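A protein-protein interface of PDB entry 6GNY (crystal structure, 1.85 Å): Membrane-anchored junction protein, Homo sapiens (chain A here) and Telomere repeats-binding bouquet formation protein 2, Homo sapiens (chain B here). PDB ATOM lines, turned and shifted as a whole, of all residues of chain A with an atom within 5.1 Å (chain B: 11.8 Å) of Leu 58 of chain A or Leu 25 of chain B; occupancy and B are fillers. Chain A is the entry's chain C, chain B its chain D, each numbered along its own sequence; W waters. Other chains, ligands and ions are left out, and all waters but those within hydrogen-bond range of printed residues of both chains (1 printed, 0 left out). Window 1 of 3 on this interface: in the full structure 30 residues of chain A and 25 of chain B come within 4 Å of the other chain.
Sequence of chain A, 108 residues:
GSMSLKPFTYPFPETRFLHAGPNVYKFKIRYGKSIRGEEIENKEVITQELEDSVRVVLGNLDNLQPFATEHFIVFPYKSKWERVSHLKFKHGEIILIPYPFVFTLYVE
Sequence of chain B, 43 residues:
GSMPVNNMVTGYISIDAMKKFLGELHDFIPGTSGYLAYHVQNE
The backbone carbonyl oxygen (O) of Gly 23 of chain B lies within hydrogen-bond range of the guanidinium group (NH1) of Arg 55 of chain A.
The backbone carbonyl oxygen (O) of His 26 of chain B lies within hydrogen-bond range of the backbone NH (N) of His 19 of chain A.
A ring nitrogen (ND1) of His 19 of chain A sits at hydrogen-bond distance from the side-chain hydroxyl (OH) of Tyr 35 of chain B.
The guanidinium group (NH1) of Arg 55 of chain A sits at hydrogen-bond distance from the backbone carbonyl oxygen (O) of Phe 21 of chain B (2.7 Å).
OG of Ser 4 of chain A lies within hydrogen-bond range of O of Leu 25 of chain B (2.9 Å).
The backbone carbonyl oxygen of Lys 19 of chain B sits at hydrogen-bond distance from the side-chain amide nitrogen of Asn 60 of chain A.
Among the printed residues, merely in contact across the chains: Arg 55 of chain A with Leu 22 of chain B, Leu 18 of chain A with His 26 of chain B, Leu 5 of chain A with Asp 27 of chain B, Arg 55 of chain A with Lys 20 of chain B, Leu 5 of chain A with Leu 25 of chain B, Val 56 of chain A with Ile 15 of chain B, Arg 55 of chain A with Leu 25 of chain B, His 19 of chain A with Leu 25 of chain B, Leu 58 of chain A with Leu 25 of chain B, Gly 59 of chain A with Lys 19 of chain B, Val 56 of chain A with Lys 19 of chain B, Val 56 of chain A with Lys 20 of chain B, Leu 5 of chain A with His 26 of chain B, Val 56 of chain A with Met 18 of chain B, Ala 20 of chain A with Leu 25 of chain B, Ala 20 of chain A with Glu 24 of chain B, Gly 59 of chain A with Phe 21 of chain B, Leu 18 of chain A with Asp 27 of chain B and Leu 58 of chain A with Phe 21 of chain B.
ND2 of Asn 60 of chain A is in hydrogen-bond range of O of Val 56 of chain A (2.8 Å).
The side-chain hydroxyl (OG) of Ser 4 of chain A sits at hydrogen-bond distance from the guanidinium group (NH2) of Arg 55 of chain A, 3.1 Å away.
N of Tyr 25 of chain A sits at hydrogen-bond distance from O of Leu 18 of chain A (2.8 Å).
Water W1 lies within hydrogen-bond range of O of Ser 4 of chain A (2.9 Å) and N of Asp 27 of chain B (2.9 Å).
Of the printed residues of chain B, Leu 5 of chain A touches Leu 25, His 26 and Asp 27.
Of chain B, only His 26 and Asp 27 come within 4 Å of Leu 18 of chain A.
Of the printed residues of chain B, His 19 of chain A touches Leu 25 (3.6 Å), His 26 (2.7 Å) and Tyr 35 (2.7 Å).
Ala 20 of chain A touches just these residues of chain B: Glu 24 (3.8 Å) and Leu 25 (3.8 Å).
No residue of chain B comes within 4 Å of Tyr 25 of chain A.
Asn 60 of chain A touches just one residue of chain B: Lys 19 (3.0 Å).
Phe 103 of chain A touches none of the printed residues of chain B.
Printed residues of chain A within 4 Å of Ile 15 of chain B: Val 56.
Of the printed residues of chain A, Lys 19 of chain B touches Val 56, Gly 59 and Asn 60.
Leu 25 of chain B touches just these residues of chain A: Ser 4 (2.9 Å), Leu 5 (3.5 Å), His 19 (3.6 Å), Ala 20 (3.8 Å), Arg 55 (3.6 Å) and Leu 58 (3.6 Å).
Of the printed residues of chain A, His 26 of chain B touches Leu 5, Leu 18 and His 19.
Ile 29 of chain B touches none of the printed residues of chain A.
Printed residues of chain A within 4 Å of Tyr 35 of chain B: His 19.
The nearest residue of chain A that does not touch Leu 25 of chain B is Leu 18 of chain A (4.1 Å).
Of the 16 printed residues of chain A, 10 touch a printed residue of chain B.
Of the 15 printed residues of chain B, 12 touch a printed residue of chain A.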
ATOM      1  N   SER A   4      -7.920  17.268 -10.839  1.00  0.00           N
ATOM      2  CA  SER A   4      -8.300  17.385  -9.439  1.00  0.00           C
ATOM      3  C   SER A   4      -7.787  18.666  -8.800  1.00  0.00           C
ATOM      4  O   SER A   4      -8.257  19.034  -7.718  1.00  0.00           O
ATOM      5  CB  SER A   4      -7.766  16.190  -8.642  1.00  0.00           C
ATOM      6  OG  SER A   4      -6.346  16.151  -8.685  1.00  0.00           O
ATOM      7  N   LEU A   5      -6.835  19.340  -9.435  1.00  0.00           N
ATOM      8  CA  LEU A   5      -6.211  20.530  -8.884  1.00  0.00           C
ATOM      9  C   LEU A   5      -6.733  21.790  -9.562  1.00  0.00           C
ATOM     10  O   LEU A   5      -7.187  21.763 -10.710  1.00  0.00           O
ATOM     11  CB  LEU A   5      -4.690  20.459  -9.036  1.00  0.00           C
ATOM     12  CG  LEU A   5      -4.048  19.216  -8.416  1.00  0.00           C
ATOM     13  CD1 LEU A   5      -2.549  19.189  -8.701  1.00  0.00           C
ATOM     14  CD2 LEU A   5      -4.325  19.165  -6.922  1.00  0.00           C
ATOM     15  N   LEU A  18       0.402  20.455  -2.037  1.00  0.00           N
ATOM     16  CA  LEU A  18      -0.450  19.377  -2.522  1.00  0.00           C
ATOM     17  C   LEU A  18      -0.577  18.294  -1.460  1.00  0.00           C
ATOM     18  O   LEU A  18       0.424  17.871  -0.871  1.00  0.00           O
ATOM     19  CB  LEU A  18       0.117  18.767  -3.809  1.00  0.00           C
ATOM     20  CG  LEU A  18       0.299  19.713  -4.997  1.00  0.00           C
ATOM     21  CD1 LEU A  18       0.984  18.983  -6.148  1.00  0.00           C
ATOM     22  CD2 LEU A  18      -1.024  20.308  -5.449  1.00  0.00           C
ATOM     23  N   HIS A  19      -1.809  17.842  -1.237  1.00  0.00           N
ATOM     24  CA  HIS A  19      -2.128  16.793  -0.275  1.00  0.00           C
ATOM     25  C   HIS A  19      -2.441  15.505  -1.024  1.00  0.00           C
ATOM     26  O   HIS A  19      -3.361  15.470  -1.847  1.00  0.00           O
ATOM     27  CB  HIS A  19      -3.316  17.204   0.599  1.00  0.00           C
ATOM     28  CG  HIS A  19      -3.886  16.082   1.414  1.00  0.00           C
ATOM     29  ND1 HIS A  19      -5.206  16.045   1.808  1.00  0.00           N
ATOM     30  CD2 HIS A  19      -3.312  14.964   1.917  1.00  0.00           C
ATOM     31  CE1 HIS A  19      -5.423  14.948   2.512  1.00  0.00           C
ATOM     32  NE2 HIS A  19      -4.289  14.274   2.590  1.00  0.00           N
ATOM     33  N   ALA A  20      -1.675  14.453  -0.744  1.00  0.00           N
ATOM     34  CA  ALA A  20      -1.951  13.132  -1.295  1.00  0.00           C
ATOM     35  C   ALA A  20      -1.779  12.112  -0.183  1.00  0.00           C
ATOM     36  O   ALA A  20      -0.690  11.991   0.387  1.00  0.00           O
ATOM     37  CB  ALA A  20      -1.023  12.811  -2.470  1.00  0.00           C
ATOM     38  N   TYR A  25       3.050  17.890  -0.045  1.00  0.00           N
ATOM     39  CA  TYR A  25       4.199  18.173  -0.896  1.00  0.00           C
ATOM     40  C   TYR A  25       4.228  19.655  -1.239  1.00  0.00           C
ATOM     41  O   TYR A  25       3.176  20.281  -1.398  1.00  0.00           O
ATOM     42  CB  TYR A  25       4.144  17.354  -2.191  1.00  0.00           C
ATOM     43  CG  TYR A  25       4.083  15.864  -1.967  1.00  0.00           C
ATOM     44  CD1 TYR A  25       2.871  15.238  -1.701  1.00  0.00           C
ATOM     45  CD2 TYR A  25       5.228  15.078  -2.027  1.00  0.00           C
ATOM     46  CE1 TYR A  25       2.801  13.872  -1.492  1.00  0.00           C
ATOM     47  CE2 TYR A  25       5.167  13.707  -1.822  1.00  0.00           C
ATOM     48  CZ  TYR A  25       3.949  13.111  -1.555  1.00  0.00           C
ATOM     49  OH  TYR A  25       3.873  11.752  -1.348  1.00  0.00           O
ATOM     50  N   PHE A  27       5.485  22.231  -4.139  1.00  0.00           N
ATOM     51  CA  PHE A  27       5.862  22.314  -5.544  1.00  0.00           C
ATOM     52  C   PHE A  27       6.063  23.767  -5.953  1.00  0.00           C
ATOM     53  O   PHE A  27       5.328  24.654  -5.509  1.00  0.00           O
ATOM     54  CB  PHE A  27       4.780  21.686  -6.436  1.00  0.00           C
ATOM     55  CG  PHE A  27       4.937  20.214  -6.635  1.00  0.00           C
ATOM     56  CD1 PHE A  27       4.575  19.327  -5.638  1.00  0.00           C
ATOM     57  CD2 PHE A  27       5.422  19.712  -7.832  1.00  0.00           C
ATOM     58  CE1 PHE A  27       4.720  17.966  -5.821  1.00  0.00           C
ATOM     59  CE2 PHE A  27       5.565  18.351  -8.021  1.00  0.00           C
ATOM     60  CZ  PHE A  27       5.213  17.478  -7.016  1.00  0.00           C
ATOM     61  N   VAL A  54       2.978  17.334 -13.003  1.00  0.00           N
ATOM     62  CA  VAL A  54       3.078  17.201 -11.552  1.00  0.00           C
ATOM     63  C   VAL A  54       2.856  15.754 -11.138  1.00  0.00           C
ATOM     64  O   VAL A  54       3.558  15.227 -10.268  1.00  0.00           O
ATOM     65  CB  VAL A  54       2.070  18.136 -10.851  1.00  0.00           C
ATOM     66  CG1 VAL A  54       1.936  17.759  -9.382  1.00  0.00           C
ATOM     67  CG2 VAL A  54       2.479  19.598 -10.995  1.00  0.00           C
ATOM     68  N   ARG A  55       1.869  15.091 -11.742  1.00  0.00           N
ATOM     69  CA  ARG A  55       1.598  13.702 -11.387  1.00  0.00           C
ATOM     70  C   ARG A  55       2.735  12.776 -11.810  1.00  0.00           C
ATOM     71  O   ARG A  55       3.011  11.784 -11.124  1.00  0.00           O
ATOM     72  CB  ARG A  55       0.278  13.252 -12.006  1.00  0.00           C
ATOM     73  CG  ARG A  55      -0.947  13.836 -11.304  1.00  0.00           C
ATOM     74  CD  ARG A  55      -2.240  13.359 -11.940  1.00  0.00           C
ATOM     75  NE  ARG A  55      -3.417  13.719 -11.151  1.00  0.00           N
ATOM     76  CZ  ARG A  55      -3.855  13.039 -10.092  1.00  0.00           C
ATOM     77  NH1 ARG A  55      -3.212  11.956  -9.676  1.00  0.00           N
ATOM     78  NH2 ARG A  55      -4.947  13.438  -9.447  1.00  0.00           N
ATOM     79  N   VAL A  56       3.409  13.073 -12.924  1.00  0.00           N
ATOM     80  CA  VAL A  56       4.572  12.273 -13.299  1.00  0.00           C
ATOM     81  C   VAL A  56       5.671  12.422 -12.254  1.00  0.00           C
ATOM     82  O   VAL A  56       6.313  11.440 -11.861  1.00  0.00           O
ATOM     83  CB  VAL A  56       5.067  12.661 -14.707  1.00  0.00           C
ATOM     84  CG1 VAL A  56       6.419  12.023 -14.992  1.00  0.00           C
ATOM     85  CG2 VAL A  56       4.050  12.240 -15.753  1.00  0.00           C
ATOM     86  N   VAL A  57       5.893  13.647 -11.774  1.00  0.00           N
ATOM     87  CA  VAL A  57       6.924  13.871 -10.764  1.00  0.00           C
ATOM     88  C   VAL A  57       6.600  13.096  -9.490  1.00  0.00           C
ATOM     89  O   VAL A  57       7.475  12.447  -8.902  1.00  0.00           O
ATOM     90  CB  VAL A  57       7.087  15.380 -10.500  1.00  0.00           C
ATOM     91  CG1 VAL A  57       7.958  15.635  -9.271  1.00  0.00           C
ATOM     92  CG2 VAL A  57       7.672  16.060 -11.729  1.00  0.00           C
ATOM     93  N   LEU A  58       5.339  13.145  -9.045  1.00  0.00           N
ATOM     94  CA  LEU A  58       4.937  12.368  -7.875  1.00  0.00           C
ATOM     95  C   LEU A  58       5.040  10.868  -8.127  1.00  0.00           C
ATOM     96  O   LEU A  58       5.186  10.091  -7.178  1.00  0.00           O
ATOM     97  CB  LEU A  58       3.508  12.726  -7.462  1.00  0.00           C
ATOM     98  CG  LEU A  58       3.307  14.136  -6.902  1.00  0.00           C
ATOM     99  CD1 LEU A  58       1.833  14.416  -6.671  1.00  0.00           C
ATOM    100  CD2 LEU A  58       4.088  14.305  -5.613  1.00  0.00           C
ATOM    101  N   GLY A  59       4.949  10.442  -9.385  1.00  0.00           N
ATOM    102  CA  GLY A  59       5.086   9.043  -9.727  1.00  0.00           C
ATOM    103  C   GLY A  59       6.509   8.558  -9.874  1.00  0.00           C
ATOM    104  O   GLY A  59       6.728   7.362 -10.087  1.00  0.00           O
ATOM    105  N   ASN A  60       7.489   9.450  -9.770  1.00  0.00           N
ATOM    106  CA  ASN A  60       8.895   9.095  -9.936  1.00  0.00           C
ATOM    107  C   ASN A  60       9.751   9.815  -8.903  1.00  0.00           C
ATOM    108  O   ASN A  60      10.831  10.328  -9.212  1.00  0.00           O
ATOM    109  CB  ASN A  60       9.366   9.407 -11.355  1.00  0.00           C
ATOM    110  CG  ASN A  60       8.647   8.573 -12.397  1.00  0.00           C
ATOM    111  OD1 ASN A  60       9.098   7.487 -12.753  1.00  0.00           O
ATOM    112  ND2 ASN A  60       7.516   9.073 -12.884  1.00  0.00           N
ATOM    113  N   LEU A  61       9.280   9.834  -7.651  1.00  0.00           N
ATOM    114  CA  LEU A  61       9.915  10.628  -6.603  1.00  0.00           C
ATOM    115  C   LEU A  61      11.399  10.316  -6.459  1.00  0.00           C
ATOM    116  O   LEU A  61      12.194  11.210  -6.145  1.00  0.00           O
ATOM    117  CB  LEU A  61       9.216  10.368  -5.265  1.00  0.00           C
ATOM    118  CG  LEU A  61       7.768  10.831  -5.106  1.00  0.00           C
ATOM    119  CD1 LEU A  61       7.167  10.229  -3.843  1.00  0.00           C
ATOM    120  CD2 LEU A  61       7.678  12.340  -5.058  1.00  0.00           C
ATOM    121  N   PHE A 103       9.877  20.282  -4.715  1.00  0.00           N
ATOM    122  CA  PHE A 103       9.977  19.960  -6.134  1.00  0.00           C
ATOM    123  C   PHE A 103       9.873  21.244  -6.946  1.00  0.00           C
ATOM    124  O   PHE A 103       8.909  22.000  -6.794  1.00  0.00           O
ATOM    125  CB  PHE A 103       8.883  18.982  -6.566  1.00  0.00           C
ATOM    126  CG  PHE A 103       9.015  17.621  -5.958  1.00  0.00           C
ATOM    127  CD1 PHE A 103       8.254  17.266  -4.859  1.00  0.00           C
ATOM    128  CD2 PHE A 103       9.900  16.695  -6.483  1.00  0.00           C
ATOM    129  CE1 PHE A 103       8.376  16.015  -4.291  1.00  0.00           C
ATOM    130  CE2 PHE A 103      10.022  15.442  -5.922  1.00  0.00           C
ATOM    131  CZ  PHE A 103       9.258  15.103  -4.824  1.00  0.00           C
ATOM    132  N   ILE B  15       6.258  12.357 -22.056  1.00  0.00           N
ATOM    133  CA  ILE B  15       5.518  12.183 -20.809  1.00  0.00           C
ATOM    134  C   ILE B  15       4.673  10.917 -20.849  1.00  0.00           C
ATOM    135  O   ILE B  15       4.447  10.277 -19.813  1.00  0.00           O
ATOM    136  CB  ILE B  15       4.649  13.427 -20.524  1.00  0.00           C
ATOM    137  CG1 ILE B  15       4.042  13.338 -19.122  1.00  0.00           C
ATOM    138  CG2 ILE B  15       3.542  13.562 -21.566  1.00  0.00           C
ATOM    139  CD1 ILE B  15       3.285  14.578 -18.697  1.00  0.00           C
ATOM    140  N   MET B  18       6.049   7.700 -19.260  1.00  0.00           N
ATOM    141  CA  MET B  18       6.445   7.790 -17.864  1.00  0.00           C
ATOM    142  C   MET B  18       5.366   7.223 -16.952  1.00  0.00           C
ATOM    143  O   MET B  18       4.172   7.287 -17.253  1.00  0.00           O
ATOM    144  CB  MET B  18       6.716   9.247 -17.475  1.00  0.00           C
ATOM    145  CG  MET B  18       7.778   9.931 -18.318  1.00  0.00           C
ATOM    146  SD  MET B  18       9.435   9.397 -17.869  1.00  0.00           S
ATOM    147  CE  MET B  18       9.733  10.411 -16.425  1.00  0.00           C
ATOM    148  N   LYS B  19       5.804   6.670 -15.823  1.00  0.00           N
ATOM    149  CA  LYS B  19       4.888   6.367 -14.733  1.00  0.00           C
ATOM    150  C   LYS B  19       4.258   7.657 -14.219  1.00  0.00           C
ATOM    151  O   LYS B  19       4.890   8.717 -14.196  1.00  0.00           O
ATOM    152  CB  LYS B  19       5.624   5.667 -13.592  1.00  0.00           C
ATOM    153  CG  LYS B  19       6.297   4.358 -13.967  1.00  0.00           C
ATOM    154  CD  LYS B  19       7.493   4.078 -13.060  1.00  0.00           C
ATOM    155  CE  LYS B  19       7.109   4.033 -11.585  1.00  0.00           C
ATOM    156  NZ  LYS B  19       8.306   3.925 -10.704  1.00  0.00           N
ATOM    157  N   LYS B  20       3.002   7.563 -13.795  1.00  0.00           N
ATOM    158  CA  LYS B  20       2.260   8.736 -13.353  1.00  0.00           C
ATOM    159  C   LYS B  20       1.454   8.373 -12.116  1.00  0.00           C
ATOM    160  O   LYS B  20       0.778   7.342 -12.100  1.00  0.00           O
ATOM    161  CB  LYS B  20       1.343   9.235 -14.478  1.00  0.00           C
ATOM    162  CG  LYS B  20       0.737  10.609 -14.264  1.00  0.00           C
ATOM    163  CD  LYS B  20      -0.122  11.035 -15.457  1.00  0.00           C
ATOM    164  CE  LYS B  20       0.690  11.107 -16.747  1.00  0.00           C
ATOM    165  NZ  LYS B  20      -0.029  11.810 -17.846  1.00  0.00           N
ATOM    166  N   PHE B  21       1.536   9.204 -11.078  1.00  0.00           N
ATOM    167  CA  PHE B  21       0.675   9.029  -9.912  1.00  0.00           C
ATOM    168  C   PHE B  21      -0.745   9.437 -10.282  1.00  0.00           C
ATOM    169  O   PHE B  21      -1.014  10.615 -10.536  1.00  0.00           O
ATOM    170  CB  PHE B  21       1.190   9.849  -8.734  1.00  0.00           C
ATOM    171  CG  PHE B  21       0.232   9.909  -7.576  1.00  0.00           C
ATOM    172  CD1 PHE B  21       0.015   8.795  -6.782  1.00  0.00           C
ATOM    173  CD2 PHE B  21      -0.455  11.076  -7.285  1.00  0.00           C
ATOM    174  CE1 PHE B  21      -0.866   8.844  -5.717  1.00  0.00           C
ATOM    175  CE2 PHE B  21      -1.339  11.131  -6.221  1.00  0.00           C
ATOM    176  CZ  PHE B  21      -1.542  10.015  -5.437  1.00  0.00           C
ATOM    177  N   LEU B  22      -1.658   8.469 -10.292  1.00  0.00           N
ATOM    178  CA  LEU B  22      -3.026   8.694 -10.735  1.00  0.00           C
ATOM    179  C   LEU B  22      -4.022   8.760  -9.585  1.00  0.00           C
ATOM    180  O   LEU B  22      -5.228   8.866  -9.836  1.00  0.00           O
ATOM    181  CB  LEU B  22      -3.443   7.591 -11.717  1.00  0.00           C
ATOM    182  CG  LEU B  22      -2.550   7.421 -12.949  1.00  0.00           C
ATOM    183  CD1 LEU B  22      -2.946   6.182 -13.741  1.00  0.00           C
ATOM    184  CD2 LEU B  22      -2.587   8.659 -13.835  1.00  0.00           C
ATOM    185  N   GLY B  23      -3.558   8.701  -8.338  1.00  0.00           N
ATOM    186  CA  GLY B  23      -4.438   8.683  -7.188  1.00  0.00           C
ATOM    187  C   GLY B  23      -4.979  10.058  -6.833  1.00  0.00           C
ATOM    188  O   GLY B  23      -4.763  11.055  -7.526  1.00  0.00           O
ATOM    189  N   GLU B  24      -5.680  10.104  -5.699  1.00  0.00           N
ATOM    190  CA  GLU B  24      -6.324  11.338  -5.261  1.00  0.00           C
ATOM    191  C   GLU B  24      -5.283  12.380  -4.874  1.00  0.00           C
ATOM    192  O   GLU B  24      -4.335  12.088  -4.139  1.00  0.00           O
ATOM    193  CB  GLU B  24      -7.251  11.067  -4.077  1.00  0.00           C
ATOM    194  CG  GLU B  24      -8.524  10.327  -4.438  1.00  0.00           C
ATOM    195  CD  GLU B  24      -9.491  10.242  -3.274  1.00  0.00           C
ATOM    196  OE1 GLU B  24      -9.155  10.749  -2.182  1.00  0.00           O
ATOM    197  OE2 GLU B  24     -10.587   9.669  -3.450  1.00  0.00           O
ATOM    198  N   LEU B  25      -5.483  13.605  -5.354  1.00  0.00           N
ATOM    199  CA  LEU B  25      -4.523  14.685  -5.176  1.00  0.00           C
ATOM    200  C   LEU B  25      -5.302  15.976  -4.968  1.00  0.00           C
ATOM    201  O   LEU B  25      -6.133  16.336  -5.808  1.00  0.00           O
ATOM    202  CB  LEU B  25      -3.600  14.775  -6.397  1.00  0.00           C
ATOM    203  CG  LEU B  25      -2.404  15.720  -6.356  1.00  0.00           C
ATOM    204  CD1 LEU B  25      -1.414  15.270  -5.295  1.00  0.00           C
ATOM    205  CD2 LEU B  25      -1.747  15.770  -7.724  1.00  0.00           C
ATOM    206  N   HIS B  26      -5.056  16.663  -3.853  1.00  0.00           N
ATOM    207  CA  HIS B  26      -5.827  17.842  -3.484  1.00  0.00           C
ATOM    208  C   HIS B  26      -4.907  19.034  -3.263  1.00  0.00           C
ATOM    209  O   HIS B  26      -3.769  18.887  -2.805  1.00  0.00           O
ATOM    210  CB  HIS B  26      -6.645  17.618  -2.199  1.00  0.00           C
ATOM    211  CG  HIS B  26      -7.422  16.341  -2.187  1.00  0.00           C
ATOM    212  ND1 HIS B  26      -8.613  16.188  -2.863  1.00  0.00           N
ATOM    213  CD2 HIS B  26      -7.186  15.161  -1.566  1.00  0.00           C
ATOM    214  CE1 HIS B  26      -9.073  14.965  -2.666  1.00  0.00           C
ATOM    215  NE2 HIS B  26      -8.225  14.322  -1.884  1.00  0.00           N
ATOM    216  N   ASP B  27      -5.419  20.220  -3.584  1.00  0.00           N
ATOM    217  CA  ASP B  27      -4.742  21.452  -3.203  1.00  0.00           C
ATOM    218  C   ASP B  27      -4.821  21.636  -1.695  1.00  0.00           C
ATOM    219  O   ASP B  27      -5.909  21.622  -1.114  1.00  0.00           O
ATOM    220  CB  ASP B  27      -5.369  22.657  -3.901  1.00  0.00           C
ATOM    221  CG  ASP B  27      -5.168  22.631  -5.397  1.00  0.00           C
ATOM    222  OD1 ASP B  27      -6.173  22.564  -6.136  1.00  0.00           O
ATOM    223  OD2 ASP B  27      -4.001  22.666  -5.833  1.00  0.00           O
ATOM    224  N   PHE B  28      -3.669  21.825  -1.064  1.00  0.00           N
ATOM    225  CA  PHE B  28      -3.619  22.093   0.371  1.00  0.00           C
ATOM    226  C   PHE B  28      -3.764  23.599   0.544  1.00  0.00           C
ATOM    227  O   PHE B  28      -2.824  24.355   0.294  1.00  0.00           O
ATOM    228  CB  PHE B  28      -2.324  21.582   0.989  1.00  0.00           C
ATOM    229  CG  PHE B  28      -2.242  21.809   2.465  1.00  0.00           C
ATOM    230  CD1 PHE B  28      -1.655  22.957   2.969  1.00  0.00           C
ATOM    231  CD2 PHE B  28      -2.807  20.903   3.353  1.00  0.00           C
ATOM    232  CE1 PHE B  28      -1.600  23.183   4.336  1.00  0.00           C
ATOM    233  CE2 PHE B  28      -2.745  21.118   4.720  1.00  0.00           C
ATOM    234  CZ  PHE B  28      -2.150  22.263   5.212  1.00  0.00           C
ATOM    235  N   ILE B  29      -4.945  24.042   0.950  1.00  0.00           N
ATOM    236  CA  ILE B  29      -5.257  25.457   1.084  1.00  0.00           C
ATOM    237  C   ILE B  29      -5.711  25.712   2.515  1.00  0.00           C
ATOM    238  O   ILE B  29      -6.841  25.395   2.885  1.00  0.00           O
ATOM    239  CB  ILE B  29      -6.334  25.892   0.073  1.00  0.00           C
ATOM    240  CG1 ILE B  29      -5.810  25.688  -1.353  1.00  0.00           C
ATOM    241  CG2 ILE B  29      -6.711  27.352   0.311  1.00  0.00           C
ATOM    242  CD1 ILE B  29      -6.854  25.827  -2.426  1.00  0.00           C
ATOM    243  N   SER B  33     -11.491  23.203   3.575  1.00  0.00           N
ATOM    244  CA  SER B  33     -11.514  21.744   3.516  1.00  0.00           C
ATOM    245  C   SER B  33     -10.874  21.108   4.748  1.00  0.00           C
ATOM    246  O   SER B  33     -10.371  19.985   4.689  1.00  0.00           O
ATOM    247  CB  SER B  33     -10.828  21.248   2.239  1.00  0.00           C
ATOM    248  OG  SER B  33     -11.182  19.906   1.956  1.00  0.00           O
ATOM    249  N   TYR B  35      -8.142  22.051   6.204  1.00  0.00           N
ATOM    250  CA  TYR B  35      -6.694  22.196   6.211  1.00  0.00           C
ATOM    251  C   TYR B  35      -6.262  23.374   7.076  1.00  0.00           C
ATOM    252  O   TYR B  35      -6.851  24.457   7.015  1.00  0.00           O
ATOM    253  CB  TYR B  35      -6.171  22.407   4.788  1.00  0.00           C
ATOM    254  CG  TYR B  35      -6.361  21.239   3.852  1.00  0.00           C
ATOM    255  CD1 TYR B  35      -5.873  19.981   4.166  1.00  0.00           C
ATOM    256  CD2 TYR B  35      -7.000  21.407   2.631  1.00  0.00           C
ATOM    257  CE1 TYR B  35      -6.037  18.920   3.304  1.00  0.00           C
ATOM    258  CE2 TYR B  35      -7.166  20.355   1.764  1.00  0.00           C
ATOM    259  CZ  TYR B  35      -6.682  19.112   2.104  1.00  0.00           C
ATOM    260  OH  TYR B  35      -6.846  18.054   1.244  1.00  0.00           O
HETATM  261  O   HOH W   1      -7.993  20.028  -4.998  1.00  0.00           O
